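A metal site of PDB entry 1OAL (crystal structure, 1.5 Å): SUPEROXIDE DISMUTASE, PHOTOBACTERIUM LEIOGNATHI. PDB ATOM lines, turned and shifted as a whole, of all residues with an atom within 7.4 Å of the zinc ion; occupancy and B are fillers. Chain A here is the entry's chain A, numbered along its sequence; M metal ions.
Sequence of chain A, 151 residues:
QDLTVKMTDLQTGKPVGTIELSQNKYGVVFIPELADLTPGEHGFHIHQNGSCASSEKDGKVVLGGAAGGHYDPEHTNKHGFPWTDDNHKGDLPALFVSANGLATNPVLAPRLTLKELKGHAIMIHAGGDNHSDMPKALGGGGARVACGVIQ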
ATOM      1  N   PHE A  44     -16.751  21.343  23.628  1.00  0.00           N
ATOM      2  CA  PHE A  44     -15.605  22.209  23.355  1.00  0.00           C
ATOM      3  C   PHE A  44     -15.901  23.521  24.077  1.00  0.00           C
ATOM      4  O   PHE A  44     -16.829  24.225  23.703  1.00  0.00           O
ATOM      5  CB  PHE A  44     -15.563  22.404  21.825  1.00  0.00           C
ATOM      6  CG  PHE A  44     -14.353  23.134  21.295  1.00  0.00           C
ATOM      7  CD1 PHE A  44     -13.083  22.898  21.778  1.00  0.00           C
ATOM      8  CD2 PHE A  44     -14.507  24.022  20.244  1.00  0.00           C
ATOM      9  CE1 PHE A  44     -11.967  23.559  21.211  1.00  0.00           C
ATOM     10  CE2 PHE A  44     -13.407  24.660  19.682  1.00  0.00           C
ATOM     11  CZ  PHE A  44     -12.158  24.448  20.199  1.00  0.00           C
ATOM     12  N   HIS A  45     -15.115  23.842  25.109  1.00  0.00           N
ATOM     13  CA  HIS A  45     -15.417  25.064  25.907  1.00  0.00           C
ATOM     14  C   HIS A  45     -14.169  25.734  26.425  1.00  0.00           C
ATOM     15  O   HIS A  45     -13.142  25.095  26.603  1.00  0.00           O
ATOM     16  CB  HIS A  45     -16.288  24.774  27.163  1.00  0.00           C
ATOM     17  CG  HIS A  45     -17.187  23.590  27.019  1.00  0.00           C
ATOM     18  ND1 HIS A  45     -16.918  22.387  27.660  1.00  0.00           N
ATOM     19  CD2 HIS A  45     -18.319  23.402  26.308  1.00  0.00           C
ATOM     20  CE1 HIS A  45     -17.876  21.517  27.361  1.00  0.00           C
ATOM     21  NE2 HIS A  45     -18.708  22.093  26.507  1.00  0.00           N
ATOM     22  N   ILE A  46     -14.276  27.032  26.674  1.00  0.00           N
ATOM     23  CA  ILE A  46     -13.243  27.760  27.427  1.00  0.00           C
ATOM     24  C   ILE A  46     -13.565  27.517  28.884  1.00  0.00           C
ATOM     25  O   ILE A  46     -14.731  27.646  29.307  1.00  0.00           O
ATOM     26  CB  ILE A  46     -13.325  29.261  27.145  1.00  0.00           C
ATOM     27  CG1 ILE A  46     -13.315  29.559  25.658  1.00  0.00           C
ATOM     28  CG2 ILE A  46     -12.172  30.007  27.877  1.00  0.00           C
ATOM     29  CD1 ILE A  46     -12.077  29.028  24.917  1.00  0.00           C
ATOM     30  N   HIS A  47     -12.556  27.146  29.646  1.00  0.00           N
ATOM     31  CA  HIS A  47     -12.690  26.987  31.110  1.00  0.00           C
ATOM     32  C   HIS A  47     -11.980  28.112  31.845  1.00  0.00           C
ATOM     33  O   HIS A  47     -11.139  28.851  31.265  1.00  0.00           O
ATOM     34  CB  HIS A  47     -12.144  25.618  31.559  1.00  0.00           C
ATOM     35  CG  HIS A  47     -13.049  24.487  31.201  1.00  0.00           C
ATOM     36  ND1 HIS A  47     -13.551  23.620  32.137  1.00  0.00           N
ATOM     37  CD2 HIS A  47     -13.563  24.097  30.007  1.00  0.00           C
ATOM     38  CE1 HIS A  47     -14.332  22.735  31.535  1.00  0.00           C
ATOM     39  NE2 HIS A  47     -14.365  23.015  30.242  1.00  0.00           N
ATOM     40  N   GLY A  69     -14.252  25.283  36.093  1.00  0.00           N
ATOM     41  CA  GLY A  69     -15.513  25.162  35.367  1.00  0.00           C
ATOM     42  C   GLY A  69     -15.492  25.927  34.064  1.00  0.00           C
ATOM     43  O   GLY A  69     -14.457  26.488  33.672  1.00  0.00           O
ATOM     44  N   HIS A  70     -16.633  25.977  33.401  1.00  0.00           N
ATOM     45  CA  HIS A  70     -16.737  26.778  32.179  1.00  0.00           C
ATOM     46  C   HIS A  70     -16.554  28.271  32.459  1.00  0.00           C
ATOM     47  O   HIS A  70     -17.063  28.822  33.493  1.00  0.00           O
ATOM     48  CB  HIS A  70     -18.087  26.521  31.476  1.00  0.00           C
ATOM     49  CG  HIS A  70     -18.244  25.105  30.989  1.00  0.00           C
ATOM     50  ND1 HIS A  70     -19.290  24.727  30.173  1.00  0.00           N
ATOM     51  CD2 HIS A  70     -17.530  23.981  31.242  1.00  0.00           C
ATOM     52  CE1 HIS A  70     -19.200  23.429  29.910  1.00  0.00           C
ATOM     53  NE2 HIS A  70     -18.137  22.956  30.553  1.00  0.00           N
ATOM     54  N   TYR A  71     -15.838  28.959  31.559  1.00  0.00           N
ATOM     55  CA  TYR A  71     -15.637  30.401  31.684  1.00  0.00           C
ATOM     56  C   TYR A  71     -17.003  31.098  31.688  1.00  0.00           C
ATOM     57  O   TYR A  71     -17.827  30.877  30.810  1.00  0.00           O
ATOM     58  CB  TYR A  71     -14.790  30.835  30.480  1.00  0.00           C
ATOM     59  CG  TYR A  71     -14.591  32.318  30.322  1.00  0.00           C
ATOM     60  CD1 TYR A  71     -14.027  33.087  31.358  1.00  0.00           C
ATOM     61  CD2 TYR A  71     -14.945  32.970  29.152  1.00  0.00           C
ATOM     62  CE1 TYR A  71     -13.815  34.459  31.211  1.00  0.00           C
ATOM     63  CE2 TYR A  71     -14.741  34.372  28.999  1.00  0.00           C
ATOM     64  CZ  TYR A  71     -14.175  35.089  30.043  1.00  0.00           C
ATOM     65  OH  TYR A  71     -13.956  36.444  29.880  1.00  0.00           O
ATOM     66  N   ASP A  72     -17.243  31.918  32.712  1.00  0.00           N
ATOM     67  CA  ASP A  72     -18.597  32.412  33.008  1.00  0.00           C
ATOM     68  C   ASP A  72     -18.488  33.783  33.667  1.00  0.00           C
ATOM     69  O   ASP A  72     -18.900  33.978  34.826  1.00  0.00           O
ATOM     70  CB  ASP A  72     -19.253  31.421  33.974  1.00  0.00           C
ATOM     71  CG  ASP A  72     -20.729  31.657  34.170  1.00  0.00           C
ATOM     72  OD1 ASP A  72     -21.362  32.394  33.375  1.00  0.00           O
ATOM     73  OD2 ASP A  72     -21.347  31.137  35.132  1.00  0.00           O
ATOM     74  N   THR A  76     -23.574  33.267  35.221  1.00  0.00           N
ATOM     75  CA  THR A  76     -24.879  32.757  34.836  1.00  0.00           C
ATOM     76  C   THR A  76     -25.151  31.434  35.487  1.00  0.00           C
ATOM     77  O   THR A  76     -26.336  31.054  35.716  1.00  0.00           O
ATOM     78  CB  THR A  76     -25.001  32.595  33.319  1.00  0.00           C
ATOM     79  OG1 THR A  76     -24.082  31.586  32.866  1.00  0.00           O
ATOM     80  CG2 THR A  76     -24.657  33.907  32.578  1.00  0.00           C
ATOM     81  N   LYS A  78     -25.095  28.616  34.158  1.00  0.00           N
ATOM     82  CA  LYS A  78     -25.909  27.822  33.247  1.00  0.00           C
ATOM     83  C   LYS A  78     -25.111  27.481  32.024  1.00  0.00           C
ATOM     84  O   LYS A  78     -24.335  28.314  31.534  1.00  0.00           O
ATOM     85  CB  LYS A  78     -27.165  28.583  32.806  1.00  0.00           C
ATOM     86  CG  LYS A  78     -28.180  28.843  33.959  1.00  0.00           C
ATOM     87  CD  LYS A  78     -29.387  29.628  33.442  1.00  0.00           C
ATOM     88  CE  LYS A  78     -30.486  29.824  34.531  1.00  0.00           C
ATOM     89  N   HIS A  79     -25.327  26.275  31.488  1.00  0.00           N
ATOM     90  CA  HIS A  79     -24.664  25.870  30.236  1.00  0.00           C
ATOM     91  C   HIS A  79     -25.649  26.005  29.066  1.00  0.00           C
ATOM     92  O   HIS A  79     -26.829  25.689  29.185  1.00  0.00           O
ATOM     93  CB  HIS A  79     -24.160  24.441  30.349  1.00  0.00           C
ATOM     94  CG  HIS A  79     -23.441  23.978  29.124  1.00  0.00           C
ATOM     95  ND1 HIS A  79     -22.189  24.452  28.760  1.00  0.00           N
ATOM     96  CD2 HIS A  79     -23.820  23.116  28.141  1.00  0.00           C
ATOM     97  CE1 HIS A  79     -21.831  23.885  27.607  1.00  0.00           C
ATOM     98  NE2 HIS A  79     -22.810  23.074  27.211  1.00  0.00           N
ATOM     99  N   GLY A  80     -25.176  26.516  27.927  1.00  0.00           N
ATOM    100  CA  GLY A  80     -26.074  26.767  26.821  1.00  0.00           C
ATOM    101  C   GLY A  80     -25.361  26.864  25.484  1.00  0.00           C
ATOM    102  O   GLY A  80     -24.378  26.174  25.250  1.00  0.00           O
ATOM    103  N   PHE A  81     -25.913  27.701  24.614  1.00  0.00           N
ATOM    104  CA  PHE A  81     -25.442  27.831  23.246  1.00  0.00           C
ATOM    105  C   PHE A  81     -24.402  28.923  23.100  1.00  0.00           C
ATOM    106  O   PHE A  81     -24.267  29.798  23.965  1.00  0.00           O
ATOM    107  CB  PHE A  81     -26.614  28.161  22.304  1.00  0.00           C
ATOM    108  CG  PHE A  81     -27.665  27.081  22.236  1.00  0.00           C
ATOM    109  CD1 PHE A  81     -27.572  26.058  21.324  1.00  0.00           C
ATOM    110  CD2 PHE A  81     -28.774  27.109  23.089  1.00  0.00           C
ATOM    111  CE1 PHE A  81     -28.570  25.078  21.237  1.00  0.00           C
ATOM    112  CE2 PHE A  81     -29.746  26.160  23.024  1.00  0.00           C
ATOM    113  CZ  PHE A  81     -29.643  25.129  22.108  1.00  0.00           C
ATOM    114  N   ASN A  87     -25.883  32.137  29.656  1.00  0.00           N
ATOM    115  CA  ASN A  87     -25.136  30.939  29.978  1.00  0.00           C
ATOM    116  C   ASN A  87     -23.665  31.217  29.801  1.00  0.00           C
ATOM    117  O   ASN A  87     -23.293  32.279  29.343  1.00  0.00           O
ATOM    118  CB  ASN A  87     -25.554  29.736  29.094  1.00  0.00           C
ATOM    119  CG  ASN A  87     -25.535  30.067  27.593  1.00  0.00           C
ATOM    120  OD1 ASN A  87     -26.506  30.601  27.053  1.00  0.00           O
ATOM    121  ND2 ASN A  87     -24.396  29.769  26.921  1.00  0.00           N
ATOM    122  N   HIS A  88     -22.834  30.243  30.128  1.00  0.00           N
ATOM    123  CA  HIS A  88     -21.361  30.468  30.156  1.00  0.00           C
ATOM    124  C   HIS A  88     -20.860  31.114  28.835  1.00  0.00           C
ATOM    125  O   HIS A  88     -21.111  30.603  27.756  1.00  0.00           O
ATOM    126  CB  HIS A  88     -20.586  29.169  30.327  1.00  0.00           C
ATOM    127  CG  HIS A  88     -21.113  28.274  31.394  1.00  0.00           C
ATOM    128  ND1 HIS A  88     -21.363  26.938  31.175  1.00  0.00           N
ATOM    129  CD2 HIS A  88     -21.407  28.519  32.688  1.00  0.00           C
ATOM    130  CE1 HIS A  88     -21.773  26.384  32.316  1.00  0.00           C
ATOM    131  NE2 HIS A  88     -21.808  27.331  33.252  1.00  0.00           N
ATOM    132  N   LYS A  89     -20.115  32.211  28.946  1.00  0.00           N
ATOM    133  CA  LYS A  89     -19.547  32.823  27.736  1.00  0.00           C
ATOM    134  C   LYS A  89     -18.517  31.846  27.123  1.00  0.00           C
ATOM    135  O   LYS A  89     -18.150  31.992  25.948  1.00  0.00           O
ATOM    136  CB  LYS A  89     -18.879  34.170  28.071  1.00  0.00           C
ATOM    137  CG  LYS A  89     -18.913  35.158  26.981  1.00  0.00           C
ATOM    138  CD  LYS A  89     -18.398  36.562  27.445  1.00  0.00           C
ATOM    139  CE  LYS A  89     -19.548  37.514  27.781  1.00  0.00           C
ATOM    140  NZ  LYS A  89     -19.129  38.952  27.552  1.00  0.00           N
ATOM    141  N   GLY A  90     -18.027  30.889  27.906  1.00  0.00           N
ATOM    142  CA  GLY A  90     -17.097  29.892  27.360  1.00  0.00           C
ATOM    143  C   GLY A  90     -17.695  28.796  26.487  1.00  0.00           C
ATOM    144  O   GLY A  90     -16.969  27.884  26.040  1.00  0.00           O
ATOM    145  N   ASP A  91     -18.999  28.836  26.274  1.00  0.00           N
ATOM    146  CA  ASP A  91     -19.668  27.759  25.523  1.00  0.00           C
ATOM    147  C   ASP A  91     -19.446  27.914  24.007  1.00  0.00           C
ATOM    148  O   ASP A  91     -20.004  28.813  23.396  1.00  0.00           O
ATOM    149  CB  ASP A  91     -21.151  27.746  25.852  1.00  0.00           C
ATOM    150  CG  ASP A  91     -21.397  27.374  27.280  1.00  0.00           C
ATOM    151  OD1 ASP A  91     -20.499  26.781  27.904  1.00  0.00           O
ATOM    152  OD2 ASP A  91     -22.514  27.566  27.836  1.00  0.00           O
ATOM    153  N   LEU A  92     -18.713  26.968  23.412  1.00  0.00           N
ATOM    154  CA  LEU A  92     -18.352  27.060  21.983  1.00  0.00           C
ATOM    155  C   LEU A  92     -19.195  26.056  21.195  1.00  0.00           C
ATOM    156  O   LEU A  92     -19.772  25.148  21.777  1.00  0.00           O
ATOM    157  CB  LEU A  92     -16.858  26.715  21.784  1.00  0.00           C
ATOM    158  CG  LEU A  92     -15.898  27.466  22.704  1.00  0.00           C
ATOM    159  CD1 LEU A  92     -14.439  26.966  22.492  1.00  0.00           C
ATOM    160  CD2 LEU A  92     -15.990  28.993  22.462  1.00  0.00           C
ATOM    161  N   ASP A 129     -22.035  17.791  23.054  1.00  0.00           N
ATOM    162  CA  ASP A 129     -22.549  18.993  23.694  1.00  0.00           C
ATOM    163  C   ASP A 129     -23.917  19.346  23.141  1.00  0.00           C
ATOM    164  O   ASP A 129     -24.043  19.820  22.011  1.00  0.00           O
ATOM    165  CB  ASP A 129     -21.576  20.172  23.506  1.00  0.00           C
ATOM    166  CG  ASP A 129     -21.876  21.328  24.454  1.00  0.00           C
ATOM    167  OD1 ASP A 129     -22.989  21.404  25.047  1.00  0.00           O
ATOM    168  OD2 ASP A 129     -21.070  22.235  24.603  1.00  0.00           O
ATOM    169  N   HIS A 131     -25.725  21.580  24.519  1.00  0.00           N
ATOM    170  CA  HIS A 131     -25.924  22.953  24.890  1.00  0.00           C
ATOM    171  C   HIS A 131     -27.056  23.114  25.893  1.00  0.00           C
ATOM    172  O   HIS A 131     -27.798  24.068  25.855  1.00  0.00           O
ATOM    173  CB  HIS A 131     -26.123  23.837  23.639  1.00  0.00           C
ATOM    174  CG  HIS A 131     -24.899  23.876  22.770  1.00  0.00           C
ATOM    175  ND1 HIS A 131     -24.823  23.252  21.534  1.00  0.00           N
ATOM    176  CD2 HIS A 131     -23.688  24.401  23.000  1.00  0.00           C
ATOM    177  CE1 HIS A 131     -23.608  23.452  21.030  1.00  0.00           C
ATOM    178  NE2 HIS A 131     -22.896  24.135  21.917  1.00  0.00           N
ATOM    179  N   ASP A 133     -28.015  21.719  30.340  1.00  0.00           N
ATOM    180  CA  ASP A 133     -27.639  20.928  31.503  1.00  0.00           C
ATOM    181  C   ASP A 133     -28.561  19.705  31.688  1.00  0.00           C
ATOM    182  O   ASP A 133     -28.438  18.969  32.706  1.00  0.00           O
ATOM    183  CB  ASP A 133     -27.672  21.790  32.754  1.00  0.00           C
ATOM    184  CG  ASP A 133     -26.527  22.731  32.804  1.00  0.00           C
ATOM    185  OD1 ASP A 133     -25.372  22.252  32.788  1.00  0.00           O
ATOM    186  OD2 ASP A 133     -26.683  23.986  32.831  1.00  0.00           O
ATOM    187  N   LEU A 138     -23.734  20.164  31.827  1.00  0.00           N
ATOM    188  CA  LEU A 138     -22.633  20.670  30.994  1.00  0.00           C
ATOM    189  C   LEU A 138     -22.638  20.064  29.587  1.00  0.00           C
ATOM    190  O   LEU A 138     -21.577  19.830  28.988  1.00  0.00           O
ATOM    191  CB  LEU A 138     -21.307  20.456  31.706  1.00  0.00           C
ATOM    192  CG  LEU A 138     -21.264  21.161  33.089  1.00  0.00           C
ATOM    193  CD1 LEU A 138     -20.041  20.693  33.869  1.00  0.00           C
ATOM    194  CD2 LEU A 138     -21.286  22.719  32.916  1.00  0.00           C
ATOM    195  N   GLY A 139     -23.831  19.825  29.088  1.00  0.00           N
ATOM    196  CA  GLY A 139     -24.037  19.373  27.716  1.00  0.00           C
ATOM    197  C   GLY A 139     -23.719  17.899  27.471  1.00  0.00           C
ATOM    198  O   GLY A 139     -23.761  17.444  26.310  1.00  0.00           O
HETATM  199 ZN    ZN M   1     -20.914  25.822  29.588  1.00  0.00          ZN
HETATM  200 CU    CU M   2     -15.511  22.063  29.001  1.00  0.00          CU
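OD2 of Asp 91 is in hydrogen-bond range of N of Gly 80 (2.9 Å). OD2 of Asp 91 sits at hydrogen-bond distance from ND2 of Asn 87 (3.0 Å). O of Lys 78 sits at hydrogen-bond distance from N of His 88. The backbone NH (N) of His 88 sits at hydrogen-bond distance from the side-chain hydroxyl (OG1) of Thr 76, 3.3 Å away. ND1 of His 45 sits close to NE2 of His 70, at 3.2 Å. NE2 of His 79 is in hydrogen-bond range of OD1 of Asp 129 (2.7 Å). The backbone NH (N) of His 79 sits at hydrogen-bond distance from the side-chain carboxylate (OD2) of Asp 133 (3.0 Å).
Of the 24 residues printed, 4 come within 4 Å of the zinc ion.
The zinc ion is bound by the side-chain carboxylate of Asp 91 (2.0 Å), a ring nitrogen (ND1) of His 88 (2.0 Å), a ring nitrogen (ND1) of His 70 (2.0 Å) and a ring nitrogen (ND1) of His 79 (2.0 Å).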
